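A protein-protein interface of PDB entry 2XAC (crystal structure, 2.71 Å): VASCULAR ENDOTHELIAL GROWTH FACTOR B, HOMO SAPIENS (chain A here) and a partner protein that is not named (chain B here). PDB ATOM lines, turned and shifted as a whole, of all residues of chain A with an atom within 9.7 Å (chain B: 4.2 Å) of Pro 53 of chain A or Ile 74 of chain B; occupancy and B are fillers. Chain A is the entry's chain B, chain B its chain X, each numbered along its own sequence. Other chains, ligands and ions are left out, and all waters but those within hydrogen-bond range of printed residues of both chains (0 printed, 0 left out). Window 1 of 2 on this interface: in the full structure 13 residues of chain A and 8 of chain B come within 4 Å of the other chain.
The side-chain carboxylate (OD2) of Asp 54 of chain A is in salt-bridge range of the guanidinium group (NE) of Arg 96 of chain B (3.2 Å).
The side-chain carboxylate of Asp 54 of chain A sits at hydrogen-bond distance from the backbone NH of Leu 57 of chain A.
The backbone NH of Lys 97 of chain A sits at hydrogen-bond distance from the backbone carbonyl oxygen of Gly 56 of chain A (3.1 Å).
The side-chain sulfur (SG) of Cys 17 of chain A is disulfide-bonded to the side-chain sulfur (SG) of Cys 59 of chain A, 2.0 Å away.
SG of Cys 52 of chain A is disulfide-bonded to SG of Cys 94 of chain A (2.0 Å).
The backbone carbonyl oxygen (O) of Gly 75 of chain B sits at hydrogen-bond distance from the backbone NH (N) of Thr 94 of chain B (2.8 Å).
The backbone NH (N) of Gly 56 of chain A sits at hydrogen-bond distance from the side-chain carboxylate (OD1) of Asp 54 of chain A, at 2.7 Å.
Pro 53 of chain A touches Ile 74 of chain B.
Pro 53 of chain A touches Gly 75 of chain B (CG to CA, 3.8 Å).
Gly 56 of chain A touches Arg 96 of chain B.
Leu 57 of chain A touches Tyr 71 of chain B (CD2 to CB, 3.97 Å).
Arg 96 of chain B touches Leu 57 of chain A (NH2 to CD2, 3.8 Å).
O of Cys 94 of chain A touches CD1 of Tyr 71 of chain B, 3.5 Å away.
Pro 96 of chain A touches Tyr 71 of chain B.
Pro 53 of chain A touches just these residues of chain B: Ile 74 (3.5 Å) and Gly 75 (3.8 Å).
Of the printed residues of chain B, Gly 56 of chain A touches Arg 96 (3.9 Å).
Of the printed residues of chain B, Leu 57 of chain A touches Tyr 71 (3.97 Å) and Arg 96 (3.8 Å).
Of the printed residues of chain B, Cys 94 of chain A touches Tyr 71 (3.5 Å).
Ile 74 of chain B touches one residue of chain A.
Of chain A, only Pro 53 comes within 4 Å of Gly 75 of chain B.
The nearest printed residue of chain B that does not touch Pro 53 of chain A is Thr 94 of chain B (5.1 Å).
The nearest residue of chain A that does not touch Ile 74 of chain B is Leu 57 of chain A (4.1 Å).
Along chain B the printed residues that touch a printed residue of chain A span positions 71 to 96.
Among the printed residues, 8 pairs touch across the chains.
Among the printed residues, Asp or Glu carboxylates within 4 Å of a Lys or Arg side-chain nitrogen of the other chain: Asp 54 of chain A with Arg 96 of chain B (3.2 Å).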
ATOM      1  N   TYR A  12     -24.759  23.467  20.108  1.00  0.00           N
ATOM      2  CA  TYR A  12     -23.443  23.987  19.766  1.00  0.00           C
ATOM      3  C   TYR A  12     -23.149  25.290  20.504  1.00  0.00           C
ATOM      4  O   TYR A  12     -22.099  25.425  21.132  1.00  0.00           O
ATOM      5  CB  TYR A  12     -23.295  24.179  18.258  1.00  0.00           C
ATOM      6  CG  TYR A  12     -22.031  24.918  17.887  1.00  0.00           C
ATOM      7  CD1 TYR A  12     -20.870  24.220  17.550  1.00  0.00           C
ATOM      8  CD2 TYR A  12     -21.990  26.313  17.885  1.00  0.00           C
ATOM      9  CE1 TYR A  12     -19.702  24.888  17.218  1.00  0.00           C
ATOM     10  CE2 TYR A  12     -20.825  26.992  17.554  1.00  0.00           C
ATOM     11  CZ  TYR A  12     -19.685  26.269  17.221  1.00  0.00           C
ATOM     12  OH  TYR A  12     -18.520  26.923  16.891  1.00  0.00           O
ATOM     13  N   ALA A  15     -22.063  24.914  24.054  1.00  0.00           N
ATOM     14  CA  ALA A  15     -21.029  23.864  24.109  1.00  0.00           C
ATOM     15  C   ALA A  15     -19.684  24.362  23.612  1.00  0.00           C
ATOM     16  O   ALA A  15     -18.741  23.579  23.467  1.00  0.00           O
ATOM     17  CB  ALA A  15     -21.441  22.647  23.307  1.00  0.00           C
ATOM     18  N   THR A  16     -19.601  25.660  23.340  1.00  0.00           N
ATOM     19  CA  THR A  16     -18.373  26.253  22.845  1.00  0.00           C
ATOM     20  C   THR A  16     -17.553  26.801  23.993  1.00  0.00           C
ATOM     21  O   THR A  16     -18.034  26.877  25.125  1.00  0.00           O
ATOM     22  CB  THR A  16     -18.655  27.377  21.836  1.00  0.00           C
ATOM     23  OG1 THR A  16     -19.873  28.040  22.192  1.00  0.00           O
ATOM     24  CG2 THR A  16     -18.782  26.810  20.431  1.00  0.00           C
ATOM     25  N   CYS A  17     -16.314  27.181  23.677  1.00  0.00           N
ATOM     26  CA  CYS A  17     -15.358  27.737  24.628  1.00  0.00           C
ATOM     27  C   CYS A  17     -15.816  29.102  25.118  1.00  0.00           C
ATOM     28  O   CYS A  17     -15.687  30.110  24.409  1.00  0.00           O
ATOM     29  CB  CYS A  17     -13.980  27.832  23.968  1.00  0.00           C
ATOM     30  SG  CYS A  17     -12.648  28.490  24.993  1.00  0.00           S
ATOM     31  N   GLY A  50     -16.163  24.357  27.960  1.00  0.00           N
ATOM     32  CA  GLY A  50     -16.594  23.978  26.630  1.00  0.00           C
ATOM     33  C   GLY A  50     -15.551  23.151  25.908  1.00  0.00           C
ATOM     34  O   GLY A  50     -14.485  22.837  26.454  1.00  0.00           O
ATOM     35  N   CYS A  51     -15.872  22.789  24.674  1.00  0.00           N
ATOM     36  CA  CYS A  51     -14.966  22.034  23.832  1.00  0.00           C
ATOM     37  C   CYS A  51     -14.693  22.803  22.551  1.00  0.00           C
ATOM     38  O   CYS A  51     -15.595  23.434  21.985  1.00  0.00           O
ATOM     39  CB  CYS A  51     -15.564  20.673  23.516  1.00  0.00           C
ATOM     40  SG  CYS A  51     -17.307  20.756  23.125  1.00  0.00           S
ATOM     41  N   CYS A  52     -13.436  22.755  22.118  1.00  0.00           N
ATOM     42  CA  CYS A  52     -12.983  23.377  20.880  1.00  0.00           C
ATOM     43  C   CYS A  52     -13.197  22.432  19.691  1.00  0.00           C
ATOM     44  O   CYS A  52     -13.472  21.246  19.895  1.00  0.00           O
ATOM     45  CB  CYS A  52     -11.508  23.762  21.003  1.00  0.00           C
ATOM     46  SG  CYS A  52     -11.203  25.164  22.074  1.00  0.00           S
ATOM     47  N   PRO A  53     -13.093  22.958  18.446  1.00  0.00           N
ATOM     48  CA  PRO A  53     -13.302  22.197  17.210  1.00  0.00           C
ATOM     49  C   PRO A  53     -12.586  20.848  17.106  1.00  0.00           C
ATOM     50  O   PRO A  53     -13.134  19.922  16.501  1.00  0.00           O
ATOM     51  CB  PRO A  53     -12.780  23.147  16.139  1.00  0.00           C
ATOM     52  CG  PRO A  53     -13.080  24.476  16.668  1.00  0.00           C
ATOM     53  CD  PRO A  53     -12.958  24.401  18.158  1.00  0.00           C
ATOM     54  N   ASP A  54     -11.380  20.742  17.661  1.00  0.00           N
ATOM     55  CA  ASP A  54     -10.596  19.517  17.601  1.00  0.00           C
ATOM     56  C   ASP A  54      -9.662  19.380  18.748  1.00  0.00           C
ATOM     57  O   ASP A  54      -9.610  20.288  19.533  1.00  0.00           O
ATOM     58  CB  ASP A  54      -9.821  19.424  16.321  1.00  0.00           C
ATOM     59  CG  ASP A  54      -8.956  20.582  16.097  1.00  0.00           C
ATOM     60  OD1 ASP A  54      -8.187  20.906  16.996  1.00  0.00           O
ATOM     61  OD2 ASP A  54      -9.019  21.153  15.014  1.00  0.00           O
ATOM     62  N   ASP A  55      -8.959  18.239  18.858  1.00  0.00           N
ATOM     63  CA  ASP A  55      -7.968  18.009  19.921  1.00  0.00           C
ATOM     64  C   ASP A  55      -6.773  18.924  19.823  1.00  0.00           C
ATOM     65  O   ASP A  55      -6.090  19.164  20.784  1.00  0.00           O
ATOM     66  CB  ASP A  55      -7.574  16.523  20.095  1.00  0.00           C
ATOM     67  CG  ASP A  55      -6.806  15.951  18.921  1.00  0.00           C
ATOM     68  OD1 ASP A  55      -6.554  16.660  17.960  1.00  0.00           O
ATOM     69  OD2 ASP A  55      -6.431  14.780  18.953  1.00  0.00           O
ATOM     70  N   GLY A  56      -6.583  19.484  18.650  1.00  0.00           N
ATOM     71  CA  GLY A  56      -5.467  20.387  18.378  1.00  0.00           C
ATOM     72  C   GLY A  56      -5.599  21.685  19.145  1.00  0.00           C
ATOM     73  O   GLY A  56      -4.607  22.248  19.616  1.00  0.00           O
ATOM     74  N   LEU A  57      -6.836  22.151  19.279  1.00  0.00           N
ATOM     75  CA  LEU A  57      -7.121  23.394  19.987  1.00  0.00           C
ATOM     76  C   LEU A  57      -7.553  23.145  21.433  1.00  0.00           C
ATOM     77  O   LEU A  57      -8.343  22.228  21.720  1.00  0.00           O
ATOM     78  CB  LEU A  57      -8.209  24.197  19.261  1.00  0.00           C
ATOM     79  CG  LEU A  57      -8.036  24.516  17.779  1.00  0.00           C
ATOM     80  CD1 LEU A  57      -9.392  24.720  17.137  1.00  0.00           C
ATOM     81  CD2 LEU A  57      -7.145  25.736  17.567  1.00  0.00           C
ATOM     82  N   GLU A  58      -7.026  23.968  22.335  1.00  0.00           N
ATOM     83  CA  GLU A  58      -7.470  23.979  23.714  1.00  0.00           C
ATOM     84  C   GLU A  58      -8.236  25.261  24.006  1.00  0.00           C
ATOM     85  O   GLU A  58      -8.032  26.289  23.344  1.00  0.00           O
ATOM     86  CB  GLU A  58      -6.290  23.822  24.677  1.00  0.00           C
ATOM     87  CG  GLU A  58      -5.270  24.956  24.686  1.00  0.00           C
ATOM     88  CD  GLU A  58      -4.227  24.803  25.789  1.00  0.00           C
ATOM     89  OE1 GLU A  58      -3.336  25.679  25.888  1.00  0.00           O
ATOM     90  OE2 GLU A  58      -4.295  23.810  26.558  1.00  0.00           O
ATOM     91  N   CYS A  59      -9.113  25.191  25.002  1.00  0.00           N
ATOM     92  CA  CYS A  59      -9.943  26.325  25.393  1.00  0.00           C
ATOM     93  C   CYS A  59      -9.314  27.100  26.551  1.00  0.00           C
ATOM     94  O   CYS A  59      -9.418  26.697  27.716  1.00  0.00           O
ATOM     95  CB  CYS A  59     -11.357  25.852  25.736  1.00  0.00           C
ATOM     96  SG  CYS A  59     -12.419  27.103  26.460  1.00  0.00           S
ATOM     97  N   GLU A  93     -11.014  31.913  24.496  1.00  0.00           N
ATOM     98  CA  GLU A  93     -10.824  31.569  23.079  1.00  0.00           C
ATOM     99  C   GLU A  93     -10.136  30.216  22.870  1.00  0.00           C
ATOM    100  O   GLU A  93      -9.419  29.736  23.752  1.00  0.00           O
ATOM    101  CB  GLU A  93     -10.060  32.677  22.332  1.00  0.00           C
ATOM    102  CG  GLU A  93      -8.535  32.583  22.389  1.00  0.00           C
ATOM    103  CD  GLU A  93      -7.846  33.565  21.455  1.00  0.00           C
ATOM    104  OE1 GLU A  93      -6.666  33.889  21.711  1.00  0.00           O
ATOM    105  OE2 GLU A  93      -8.475  34.012  20.467  1.00  0.00           O
ATOM    106  N   CYS A  94     -10.355  29.620  21.696  1.00  0.00           N
ATOM    107  CA  CYS A  94      -9.682  28.380  21.295  1.00  0.00           C
ATOM    108  C   CYS A  94      -8.296  28.640  20.684  1.00  0.00           C
ATOM    109  O   CYS A  94      -8.176  29.167  19.575  1.00  0.00           O
ATOM    110  CB  CYS A  94     -10.545  27.575  20.317  1.00  0.00           C
ATOM    111  SG  CYS A  94     -11.986  26.743  21.044  1.00  0.00           S
ATOM    112  N   ARG A  95      -7.257  28.267  21.428  1.00  0.00           N
ATOM    113  CA  ARG A  95      -5.871  28.432  20.991  1.00  0.00           C
ATOM    114  C   ARG A  95      -5.239  27.079  20.732  1.00  0.00           C
ATOM    115  O   ARG A  95      -5.571  26.110  21.416  1.00  0.00           O
ATOM    116  CB  ARG A  95      -5.048  29.138  22.065  1.00  0.00           C
ATOM    117  CG  ARG A  95      -5.188  30.631  22.099  1.00  0.00           C
ATOM    118  CD  ARG A  95      -4.052  31.227  22.898  1.00  0.00           C
ATOM    119  NE  ARG A  95      -4.107  32.684  22.929  1.00  0.00           N
ATOM    120  CZ  ARG A  95      -3.283  33.449  23.639  1.00  0.00           C
ATOM    121  NH1 ARG A  95      -3.415  34.769  23.602  1.00  0.00           N
ATOM    122  NH2 ARG A  95      -2.332  32.898  24.391  1.00  0.00           N
ATOM    123  N   PRO A  96      -4.305  27.009  19.767  1.00  0.00           N
ATOM    124  CA  PRO A  96      -3.605  25.752  19.536  1.00  0.00           C
ATOM    125  C   PRO A  96      -2.730  25.408  20.730  1.00  0.00           C
ATOM    126  O   PRO A  96      -2.109  26.292  21.315  1.00  0.00           O
ATOM    127  CB  PRO A  96      -2.735  26.046  18.307  1.00  0.00           C
ATOM    128  CG  PRO A  96      -3.260  27.340  17.733  1.00  0.00           C
ATOM    129  CD  PRO A  96      -3.801  28.085  18.896  1.00  0.00           C
ATOM    130  N   LYS A  97      -2.703  24.130  21.095  1.00  0.00           N
ATOM    131  CA  LYS A  97      -1.883  23.654  22.209  1.00  0.00           C
ATOM    132  C   LYS A  97      -0.392  23.814  21.916  1.00  0.00           C
ATOM    133  O   LYS A  97       0.080  23.503  20.818  1.00  0.00           O
ATOM    134  CB  LYS A  97      -2.216  22.199  22.548  1.00  0.00           C
ATOM    135  CG  LYS A  97      -3.632  22.001  23.077  1.00  0.00           C
ATOM    136  CD  LYS A  97      -4.055  20.533  23.065  1.00  0.00           C
ATOM    137  CE  LYS A  97      -5.487  20.359  23.560  1.00  0.00           C
ATOM    138  NZ  LYS A  97      -5.630  20.705  25.005  1.00  0.00           N
ATOM    139  N   MET B  20     -11.089  23.102   5.640  1.00  0.00           N
ATOM    140  CA  MET B  20     -10.086  24.178   5.618  1.00  0.00           C
ATOM    141  C   MET B  20      -8.696  23.731   6.093  1.00  0.00           C
ATOM    142  O   MET B  20      -8.527  22.623   6.615  1.00  0.00           O
ATOM    143  CB  MET B  20     -10.571  25.433   6.375  1.00  0.00           C
ATOM    144  CG  MET B  20     -10.645  25.318   7.901  1.00  0.00           C
ATOM    145  SD  MET B  20      -9.251  26.039   8.808  1.00  0.00           S
ATOM    146  CE  MET B  20      -9.726  27.752   8.932  1.00  0.00           C
ATOM    147  N   THR B  70      -6.295  31.364   9.630  1.00  0.00           N
ATOM    148  CA  THR B  70      -5.661  31.126  10.927  1.00  0.00           C
ATOM    149  C   THR B  70      -6.435  30.063  11.703  1.00  0.00           C
ATOM    150  O   THR B  70      -7.384  29.467  11.181  1.00  0.00           O
ATOM    151  CB  THR B  70      -5.583  32.421  11.782  1.00  0.00           C
ATOM    152  OG1 THR B  70      -6.861  32.692  12.372  1.00  0.00           O
ATOM    153  CG2 THR B  70      -5.128  33.625  10.948  1.00  0.00           C
ATOM    154  N   TYR B  71      -6.023  29.829  12.948  1.00  0.00           N
ATOM    155  CA  TYR B  71      -6.730  28.918  13.840  1.00  0.00           C
ATOM    156  C   TYR B  71      -8.037  29.537  14.302  1.00  0.00           C
ATOM    157  O   TYR B  71      -9.013  28.825  14.540  1.00  0.00           O
ATOM    158  CB  TYR B  71      -5.864  28.525  15.045  1.00  0.00           C
ATOM    159  CG  TYR B  71      -5.336  29.687  15.864  1.00  0.00           C
ATOM    160  CD1 TYR B  71      -6.065  30.205  16.935  1.00  0.00           C
ATOM    161  CD2 TYR B  71      -4.097  30.255  15.575  1.00  0.00           C
ATOM    162  CE1 TYR B  71      -5.580  31.267  17.689  1.00  0.00           C
ATOM    163  CE2 TYR B  71      -3.601  31.315  16.324  1.00  0.00           C
ATOM    164  CZ  TYR B  71      -4.346  31.816  17.377  1.00  0.00           C
ATOM    165  OH  TYR B  71      -3.845  32.860  18.113  1.00  0.00           O
ATOM    166  N   LYS B  72      -8.042  30.868  14.417  1.00  0.00           N
ATOM    167  CA  LYS B  72      -9.231  31.635  14.807  1.00  0.00           C
ATOM    168  C   LYS B  72     -10.421  31.288  13.923  1.00  0.00           C
ATOM    169  O   LYS B  72     -11.558  31.328  14.370  1.00  0.00           O
ATOM    170  CB  LYS B  72      -8.965  33.146  14.732  1.00  0.00           C
ATOM    171  CG  LYS B  72      -7.899  33.672  15.691  1.00  0.00           C
ATOM    172  CD  LYS B  72      -7.623  35.164  15.471  1.00  0.00           C
ATOM    173  CE  LYS B  72      -6.859  35.443  14.160  1.00  0.00           C
ATOM    174  NZ  LYS B  72      -5.483  34.855  14.142  1.00  0.00           N
ATOM    175  N   GLU B  73     -10.137  30.930  12.675  1.00  0.00           N
ATOM    176  CA  GLU B  73     -11.165  30.603  11.695  1.00  0.00           C
ATOM    177  C   GLU B  73     -11.668  29.160  11.741  1.00  0.00           C
ATOM    178  O   GLU B  73     -12.553  28.805  10.967  1.00  0.00           O
ATOM    179  CB  GLU B  73     -10.680  30.937  10.281  1.00  0.00           C
ATOM    180  CG  GLU B  73     -10.726  32.414   9.939  1.00  0.00           C
ATOM    181  CD  GLU B  73      -9.554  33.176  10.504  1.00  0.00           C
ATOM    182  OE1 GLU B  73      -8.463  33.093   9.909  1.00  0.00           O
ATOM    183  OE2 GLU B  73      -9.728  33.862  11.536  1.00  0.00           O
ATOM    184  N   ILE B  74     -11.105  28.333  12.625  1.00  0.00           N
ATOM    185  CA  ILE B  74     -11.586  26.955  12.792  1.00  0.00           C
ATOM    186  C   ILE B  74     -12.771  26.950  13.750  1.00  0.00           C
ATOM    187  O   ILE B  74     -12.676  27.451  14.880  1.00  0.00           O
ATOM    188  CB  ILE B  74     -10.501  25.966  13.314  1.00  0.00           C
ATOM    189  CG1 ILE B  74      -9.170  26.145  12.581  1.00  0.00           C
ATOM    190  CG2 ILE B  74     -10.988  24.508  13.191  1.00  0.00           C
ATOM    191  CD1 ILE B  74      -7.992  25.591  13.336  1.00  0.00           C
ATOM    192  N   GLY B  75     -13.875  26.372  13.291  1.00  0.00           N
ATOM    193  CA  GLY B  75     -15.134  26.372  14.031  1.00  0.00           C
ATOM    194  C   GLY B  75     -16.282  26.851  13.161  1.00  0.00           C
ATOM    195  O   GLY B  75     -16.227  26.746  11.934  1.00  0.00           O
ATOM    196  N   THR B  94     -16.240  25.020   9.735  1.00  0.00           N
ATOM    197  CA  THR B  94     -14.916  24.726   9.199  1.00  0.00           C
ATOM    198  C   THR B  94     -14.161  23.732  10.079  1.00  0.00           C
ATOM    199  O   THR B  94     -14.268  23.757  11.309  1.00  0.00           O
ATOM    200  CB  THR B  94     -14.069  25.997   8.993  1.00  0.00           C
ATOM    201  OG1 THR B  94     -13.705  26.547  10.263  1.00  0.00           O
ATOM    202  CG2 THR B  94     -14.832  27.034   8.182  1.00  0.00           C
ATOM    203  N   ARG B  96     -10.206  21.233  10.116  1.00  0.00           N
ATOM    204  CA  ARG B  96      -8.941  20.839   9.525  1.00  0.00           C
ATOM    205  C   ARG B  96      -8.704  19.362   9.790  1.00  0.00           C
ATOM    206  O   ARG B  96      -9.453  18.715  10.534  1.00  0.00           O
ATOM    207  CB  ARG B  96      -7.796  21.675  10.099  1.00  0.00           C
ATOM    208  CG  ARG B  96      -7.782  21.733  11.617  1.00  0.00           C
ATOM    209  CD  ARG B  96      -6.656  22.583  12.120  1.00  0.00           C
ATOM    210  NE  ARG B  96      -6.782  22.848  13.550  1.00  0.00           N
ATOM    211  CZ  ARG B  96      -5.802  23.328  14.312  1.00  0.00           C
ATOM    212  NH1 ARG B  96      -5.085  22.515  15.077  1.00  0.00           N
ATOM    213  NH2 ARG B  96      -5.544  24.628  14.319  1.00  0.00           N
